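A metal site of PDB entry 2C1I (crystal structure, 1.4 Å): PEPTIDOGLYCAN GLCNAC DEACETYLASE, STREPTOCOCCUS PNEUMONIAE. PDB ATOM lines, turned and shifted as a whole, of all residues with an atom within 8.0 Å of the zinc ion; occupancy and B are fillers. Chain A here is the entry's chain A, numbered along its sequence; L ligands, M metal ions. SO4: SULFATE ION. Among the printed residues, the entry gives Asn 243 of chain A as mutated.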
ATOM      1  N   PHE A 242     -18.327   5.262  11.359  1.00  0.00           N
ATOM      2  CA  PHE A 242     -18.232   4.229  12.413  1.00  0.00           C
ATOM      3  C   PHE A 242     -19.617   3.805  12.815  1.00  0.00           C
ATOM      4  O   PHE A 242     -20.407   4.663  13.239  1.00  0.00           O
ATOM      5  CB  PHE A 242     -17.511   4.799  13.643  1.00  0.00           C
ATOM      6  CG  PHE A 242     -16.051   5.117  13.412  1.00  0.00           C
ATOM      7  CD1 PHE A 242     -15.100   4.123  13.458  1.00  0.00           C
ATOM      8  CD2 PHE A 242     -15.661   6.422  13.148  1.00  0.00           C
ATOM      9  CE1 PHE A 242     -13.769   4.429  13.215  1.00  0.00           C
ATOM     10  CE2 PHE A 242     -14.335   6.715  12.903  1.00  0.00           C
ATOM     11  CZ  PHE A 242     -13.400   5.702  12.921  1.00  0.00           C
ATOM     12  N   ASN A 243     -19.895   2.496  12.723  1.00  0.00           N
ATOM     13  CA  ASN A 243     -21.187   1.960  13.131  1.00  0.00           C
ATOM     14  C   ASN A 243     -21.177   1.335  14.522  1.00  0.00           C
ATOM     15  O   ASN A 243     -20.149   0.776  14.960  1.00  0.00           O
ATOM     16  CB  ASN A 243     -21.570   0.802  12.187  1.00  0.00           C
ATOM     17  CG  ASN A 243     -22.125   1.271  10.866  1.00  0.00           C
ATOM     18  OD1 ASN A 243     -22.105   2.469  10.513  1.00  0.00           O
ATOM     19  ND2 ASN A 243     -22.678   0.317  10.102  1.00  0.00           N
ATOM     20  N   ASP A 244     -22.345   1.370  15.163  1.00  0.00           N
ATOM     21  CA  ASP A 244     -22.737   0.466  16.254  1.00  0.00           C
ATOM     22  C   ASP A 244     -22.480   1.014  17.637  1.00  0.00           C
ATOM     23  O   ASP A 244     -22.844   0.360  18.639  1.00  0.00           O
ATOM     24  CB  ASP A 244     -22.222  -0.981  16.149  1.00  0.00           C
ATOM     25  CG  ASP A 244     -22.645  -1.684  14.895  1.00  0.00           C
ATOM     26  OD1 ASP A 244     -23.617  -1.325  14.230  1.00  0.00           O
ATOM     27  OD2 ASP A 244     -21.943  -2.665  14.545  1.00  0.00           O
ATOM     28  N   GLY A 245     -21.918   2.217  17.745  1.00  0.00           N
ATOM     29  CA  GLY A 245     -21.665   2.784  19.056  1.00  0.00           C
ATOM     30  C   GLY A 245     -22.865   3.511  19.617  1.00  0.00           C
ATOM     31  O   GLY A 245     -23.994   3.319  19.187  1.00  0.00           O
ATOM     32  N   PHE A 268     -22.573   6.429  13.184  1.00  0.00           N
ATOM     33  CA  PHE A 268     -23.955   5.940  13.072  1.00  0.00           C
ATOM     34  C   PHE A 268     -24.224   5.092  14.293  1.00  0.00           C
ATOM     35  O   PHE A 268     -23.753   3.947  14.410  1.00  0.00           O
ATOM     36  CB  PHE A 268     -24.135   5.154  11.760  1.00  0.00           C
ATOM     37  CG  PHE A 268     -24.118   6.068  10.549  1.00  0.00           C
ATOM     38  CD1 PHE A 268     -25.284   6.766  10.188  1.00  0.00           C
ATOM     39  CD2 PHE A 268     -22.941   6.285   9.834  1.00  0.00           C
ATOM     40  CE1 PHE A 268     -25.278   7.656   9.097  1.00  0.00           C
ATOM     41  CE2 PHE A 268     -22.943   7.151   8.759  1.00  0.00           C
ATOM     42  CZ  PHE A 268     -24.097   7.831   8.389  1.00  0.00           C
ATOM     43  N   VAL A 269     -24.961   5.680  15.232  1.00  0.00           N
ATOM     44  CA  VAL A 269     -25.113   5.092  16.543  1.00  0.00           C
ATOM     45  C   VAL A 269     -26.441   4.360  16.695  1.00  0.00           C
ATOM     46  O   VAL A 269     -27.442   4.674  16.037  1.00  0.00           O
ATOM     47  CB  VAL A 269     -24.925   6.127  17.696  1.00  0.00           C
ATOM     48  CG1 VAL A 269     -23.542   6.753  17.613  1.00  0.00           C
ATOM     49  CG2 VAL A 269     -26.005   7.186  17.668  1.00  0.00           C
ATOM     50  N   LEU A 270     -26.451   3.365  17.583  1.00  0.00           N
ATOM     51  CA  LEU A 270     -27.680   2.647  17.916  1.00  0.00           C
ATOM     52  C   LEU A 270     -28.429   3.321  19.031  1.00  0.00           C
ATOM     53  O   LEU A 270     -27.866   3.655  20.065  1.00  0.00           O
ATOM     54  CB  LEU A 270     -27.329   1.208  18.362  1.00  0.00           C
ATOM     55  CG  LEU A 270     -26.928   0.285  17.202  1.00  0.00           C
ATOM     56  CD1 LEU A 270     -26.193  -0.975  17.740  1.00  0.00           C
ATOM     57  CD2 LEU A 270     -28.143  -0.106  16.404  1.00  0.00           C
ATOM     58  N   HIS A 294     -28.529   4.663  13.400  1.00  0.00           N
ATOM     59  CA  HIS A 294     -28.248   3.302  12.923  1.00  0.00           C
ATOM     60  C   HIS A 294     -29.343   2.318  13.365  1.00  0.00           C
ATOM     61  O   HIS A 294     -29.045   1.131  13.441  1.00  0.00           O
ATOM     62  CB  HIS A 294     -26.887   2.834  13.447  1.00  0.00           C
ATOM     63  CG  HIS A 294     -26.322   1.634  12.763  1.00  0.00           C
ATOM     64  ND1 HIS A 294     -26.415   1.407  11.396  1.00  0.00           N
ATOM     65  CD2 HIS A 294     -25.616   0.578  13.262  1.00  0.00           C
ATOM     66  CE1 HIS A 294     -25.784   0.278  11.101  1.00  0.00           C
ATOM     67  NE2 HIS A 294     -25.299  -0.248  12.212  1.00  0.00           N
ATOM     68  N   SER A 295     -30.557   2.836  13.623  1.00  0.00           N
ATOM     69  CA  SER A 295     -31.689   2.079  14.174  1.00  0.00           C
ATOM     70  C   SER A 295     -31.590   2.018  15.679  1.00  0.00           C
ATOM     71  O   SER A 295     -30.593   2.441  16.283  1.00  0.00           O
ATOM     72  CB  SER A 295     -31.892   0.703  13.591  1.00  0.00           C
ATOM     73  OG  SER A 295     -31.059  -0.285  14.191  1.00  0.00           O
ATOM     74  N   HIS A 298     -30.657  -2.605  15.969  1.00  0.00           N
ATOM     75  CA  HIS A 298     -29.903  -3.340  14.945  1.00  0.00           C
ATOM     76  C   HIS A 298     -30.649  -4.538  14.302  1.00  0.00           C
ATOM     77  O   HIS A 298     -30.016  -5.495  13.921  1.00  0.00           O
ATOM     78  CB  HIS A 298     -28.548  -3.821  15.498  1.00  0.00           C
ATOM     79  CG  HIS A 298     -27.453  -3.799  14.491  1.00  0.00           C
ATOM     80  ND1 HIS A 298     -27.180  -4.836  13.625  1.00  0.00           N
ATOM     81  CD2 HIS A 298     -26.540  -2.836  14.189  1.00  0.00           C
ATOM     82  CE1 HIS A 298     -26.149  -4.520  12.843  1.00  0.00           C
ATOM     83  NE2 HIS A 298     -25.729  -3.296  13.183  1.00  0.00           N
ATOM     84  N   PRO A 299     -31.972  -4.450  14.063  1.00  0.00           N
ATOM     85  CA  PRO A 299     -32.627  -5.535  13.325  1.00  0.00           C
ATOM     86  C   PRO A 299     -32.329  -5.389  11.831  1.00  0.00           C
ATOM     87  O   PRO A 299     -31.826  -4.334  11.375  1.00  0.00           O
ATOM     88  CB  PRO A 299     -34.110  -5.241  13.608  1.00  0.00           C
ATOM     89  CG  PRO A 299     -34.164  -3.750  13.603  1.00  0.00           C
ATOM     90  CD  PRO A 299     -32.897  -3.317  14.338  1.00  0.00           C
ATOM     91  N   ARG A 332     -28.214   5.179   8.560  1.00  0.00           N
ATOM     92  CA  ARG A 332     -27.583   4.041   7.904  1.00  0.00           C
ATOM     93  C   ARG A 332     -28.271   2.742   8.336  1.00  0.00           C
ATOM     94  O   ARG A 332     -28.186   2.362   9.515  1.00  0.00           O
ATOM     95  CB  ARG A 332     -26.077   3.935   8.232  1.00  0.00           C
ATOM     96  CG  ARG A 332     -25.474   2.677   7.606  1.00  0.00           C
ATOM     97  CD  ARG A 332     -23.959   2.690   7.739  1.00  0.00           C
ATOM     98  NE  ARG A 332     -23.348   3.672   6.865  1.00  0.00           N
ATOM     99  CZ  ARG A 332     -22.076   4.050   7.003  1.00  0.00           C
ATOM    100  NH1 ARG A 332     -21.346   3.661   8.072  1.00  0.00           N
ATOM    101  NH2 ARG A 332     -21.531   4.850   6.119  1.00  0.00           N
ATOM    102  N   PRO A 333     -28.958   2.064   7.422  1.00  0.00           N
ATOM    103  CA  PRO A 333     -29.574   0.761   7.761  1.00  0.00           C
ATOM    104  C   PRO A 333     -28.583  -0.315   8.170  1.00  0.00           C
ATOM    105  O   PRO A 333     -27.633  -0.578   7.422  1.00  0.00           O
ATOM    106  CB  PRO A 333     -30.314   0.389   6.474  1.00  0.00           C
ATOM    107  CG  PRO A 333     -30.588   1.757   5.781  1.00  0.00           C
ATOM    108  CD  PRO A 333     -29.306   2.501   6.049  1.00  0.00           C
ATOM    109  N   PRO A 334     -28.822  -1.000   9.304  1.00  0.00           N
ATOM    110  CA  PRO A 334     -28.054  -2.229   9.623  1.00  0.00           C
ATOM    111  C   PRO A 334     -28.026  -3.173   8.435  1.00  0.00           C
ATOM    112  O   PRO A 334     -29.062  -3.407   7.777  1.00  0.00           O
ATOM    113  CB  PRO A 334     -28.812  -2.820  10.832  1.00  0.00           C
ATOM    114  CG  PRO A 334     -29.431  -1.590  11.471  1.00  0.00           C
ATOM    115  CD  PRO A 334     -29.818  -0.685  10.329  1.00  0.00           C
ATOM    116  N   TYR A 335     -26.847  -3.696   8.154  1.00  0.00           N
ATOM    117  CA  TYR A 335     -26.649  -4.693   7.100  1.00  0.00           C
ATOM    118  C   TYR A 335     -26.889  -4.112   5.703  1.00  0.00           C
ATOM    119  O   TYR A 335     -26.846  -4.848   4.723  1.00  0.00           O
ATOM    120  CB  TYR A 335     -27.528  -5.981   7.323  1.00  0.00           C
ATOM    121  CG  TYR A 335     -27.528  -6.458   8.748  1.00  0.00           C
ATOM    122  CD1 TYR A 335     -26.419  -7.132   9.263  1.00  0.00           C
ATOM    123  CD2 TYR A 335     -28.611  -6.217   9.599  1.00  0.00           C
ATOM    124  CE1 TYR A 335     -26.390  -7.555  10.577  1.00  0.00           C
ATOM    125  CE2 TYR A 335     -28.578  -6.649  10.913  1.00  0.00           C
ATOM    126  CZ  TYR A 335     -27.479  -7.307  11.405  1.00  0.00           C
ATOM    127  OH  TYR A 335     -27.442  -7.661  12.741  1.00  0.00           O
ATOM    128  N   GLY A 336     -27.137  -2.794   5.615  1.00  0.00           N
ATOM    129  CA  GLY A 336     -27.494  -2.218   4.318  1.00  0.00           C
ATOM    130  C   GLY A 336     -28.903  -2.597   3.871  1.00  0.00           C
ATOM    131  O   GLY A 336     -29.281  -2.375   2.706  1.00  0.00           O
ATOM    132  N   TRP A 353     -22.288   2.885   1.937  1.00  0.00           N
ATOM    133  CA  TRP A 353     -20.819   3.016   1.899  1.00  0.00           C
ATOM    134  C   TRP A 353     -20.352   2.368   0.612  1.00  0.00           C
ATOM    135  O   TRP A 353     -21.118   1.641  -0.005  1.00  0.00           O
ATOM    136  CB  TRP A 353     -20.166   2.314   3.108  1.00  0.00           C
ATOM    137  CG  TRP A 353     -20.472   0.833   3.167  1.00  0.00           C
ATOM    138  CD1 TRP A 353     -19.714  -0.193   2.629  1.00  0.00           C
ATOM    139  CD2 TRP A 353     -21.595   0.223   3.801  1.00  0.00           C
ATOM    140  NE1 TRP A 353     -20.325  -1.409   2.884  1.00  0.00           N
ATOM    141  CE2 TRP A 353     -21.469  -1.176   3.597  1.00  0.00           C
ATOM    142  CE3 TRP A 353     -22.692   0.716   4.518  1.00  0.00           C
ATOM    143  CZ2 TRP A 353     -22.404  -2.078   4.101  1.00  0.00           C
ATOM    144  CZ3 TRP A 353     -23.617  -0.170   5.037  1.00  0.00           C
ATOM    145  CH2 TRP A 353     -23.491  -1.560   4.791  1.00  0.00           C
ATOM    146  N   LEU A 383     -16.557   2.203   5.755  1.00  0.00           N
ATOM    147  CA  LEU A 383     -17.248   1.585   6.878  1.00  0.00           C
ATOM    148  C   LEU A 383     -16.260   0.957   7.876  1.00  0.00           C
ATOM    149  O   LEU A 383     -15.458   0.095   7.487  1.00  0.00           O
ATOM    150  CB  LEU A 383     -18.216   0.501   6.355  1.00  0.00           C
ATOM    151  CG  LEU A 383     -18.905  -0.335   7.453  1.00  0.00           C
ATOM    152  CD1 LEU A 383     -19.814   0.515   8.324  1.00  0.00           C
ATOM    153  CD2 LEU A 383     -19.688  -1.494   6.802  1.00  0.00           C
ATOM    154  N   MET A 384     -16.348   1.397   9.136  1.00  0.00           N
ATOM    155  CA  MET A 384     -15.688   0.762  10.281  1.00  0.00           C
ATOM    156  C   MET A 384     -16.681   0.613  11.380  1.00  0.00           C
ATOM    157  O   MET A 384     -17.786   1.180  11.320  1.00  0.00           O
ATOM    158  CB  MET A 384     -14.523   1.613  10.734  1.00  0.00           C
ATOM    159  CG  MET A 384     -13.354   1.655   9.690  1.00  0.00           C
ATOM    160  SD  MET A 384     -11.965   2.606  10.260  1.00  0.00           S
ATOM    161  CE  MET A 384     -10.788   2.340   8.972  1.00  0.00           C
ATOM    162  N   HIS A 385     -16.281  -0.104  12.421  1.00  0.00           N
ATOM    163  CA  HIS A 385     -17.150  -0.351  13.613  1.00  0.00           C
ATOM    164  C   HIS A 385     -16.313   0.029  14.816  1.00  0.00           C
ATOM    165  O   HIS A 385     -15.316  -0.658  15.060  1.00  0.00           O
ATOM    166  CB  HIS A 385     -17.570  -1.838  13.645  1.00  0.00           C
ATOM    167  CG  HIS A 385     -18.328  -2.282  12.429  1.00  0.00           C
ATOM    168  ND1 HIS A 385     -17.717  -2.572  11.229  1.00  0.00           N
ATOM    169  CD2 HIS A 385     -19.658  -2.436  12.213  1.00  0.00           C
ATOM    170  CE1 HIS A 385     -18.624  -2.876  10.308  1.00  0.00           C
ATOM    171  NE2 HIS A 385     -19.815  -2.819  10.892  1.00  0.00           N
ATOM    172  N   ILE A 387     -16.292  -0.452  17.887  1.00  0.00           N
ATOM    173  CA  ILE A 387     -16.727  -1.210  19.044  1.00  0.00           C
ATOM    174  C   ILE A 387     -15.736  -2.286  19.453  1.00  0.00           C
ATOM    175  O   ILE A 387     -15.936  -2.891  20.514  1.00  0.00           O
ATOM    176  CB  ILE A 387     -18.246  -1.661  18.913  1.00  0.00           C
ATOM    177  CG1 ILE A 387     -18.517  -2.441  17.625  1.00  0.00           C
ATOM    178  CG2 ILE A 387     -19.182  -0.418  18.964  1.00  0.00           C
ATOM    179  CD1 ILE A 387     -18.841  -1.531  16.462  1.00  0.00           C
HETATM  180  S   SO4 L   1     -23.318  -3.423  10.100  1.00  0.00           S
HETATM  181  O1  SO4 L   1     -23.788  -4.719  10.782  1.00  0.00           O
HETATM  182  O2  SO4 L   1     -24.415  -3.070   9.130  1.00  0.00           O
HETATM  183  O3  SO4 L   1     -23.095  -2.364  11.129  1.00  0.00           O
HETATM  184  O4  SO4 L   1     -21.969  -3.673   9.504  1.00  0.00           O
HETATM  185 ZN    ZN M   1     -24.321  -1.996  12.582  1.00  0.00          ZN
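O of Arg 332 is in hydrogen-bond range of ND1 of His 294 (2.8 Å). A ring nitrogen (NE2) of His 294 sits close to the side-chain amide nitrogen (ND2) of Asn 243, 3.4 Å away. The backbone NH of Asp 244 lies within hydrogen-bond range of the backbone carbonyl oxygen of Phe 268 (3.0 Å). The side-chain hydroxyl (OH) of Tyr 335 is in hydrogen-bond range of a ring nitrogen (ND1) of His 298. The side-chain amide oxygen of Asn 243 is in hydrogen-bond range of the guanidinium group of Arg 332 (2.8 Å). The backbone NH (N) of Asn 243 lies within hydrogen-bond range of the backbone carbonyl oxygen (O) of Met 384 (2.9 Å). The backbone NH (N) of His 294 sits at hydrogen-bond distance from the backbone carbonyl oxygen (O) of Val 269, at 2.9 Å. OG of Ser 295 is in hydrogen-bond range of N of His 298, 3.0 Å away.
Merely in contact with the zinc ion: Asn 243. Within 4 Å of the zinc ion: Asn 243, Asp 244, His 294 and His 298. The nearest printed residue that does not touch the zinc ion is His 385 (4.7 Å).
The zinc ion is bound by OD1 of Asp 244 (1.9 Å), O3 of the ligand (1.9 Å), NE2 of His 298 (2.0 Å) and NE2 of His 294 (2.0 Å). The zinc ion has four donor atoms within binding distance.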
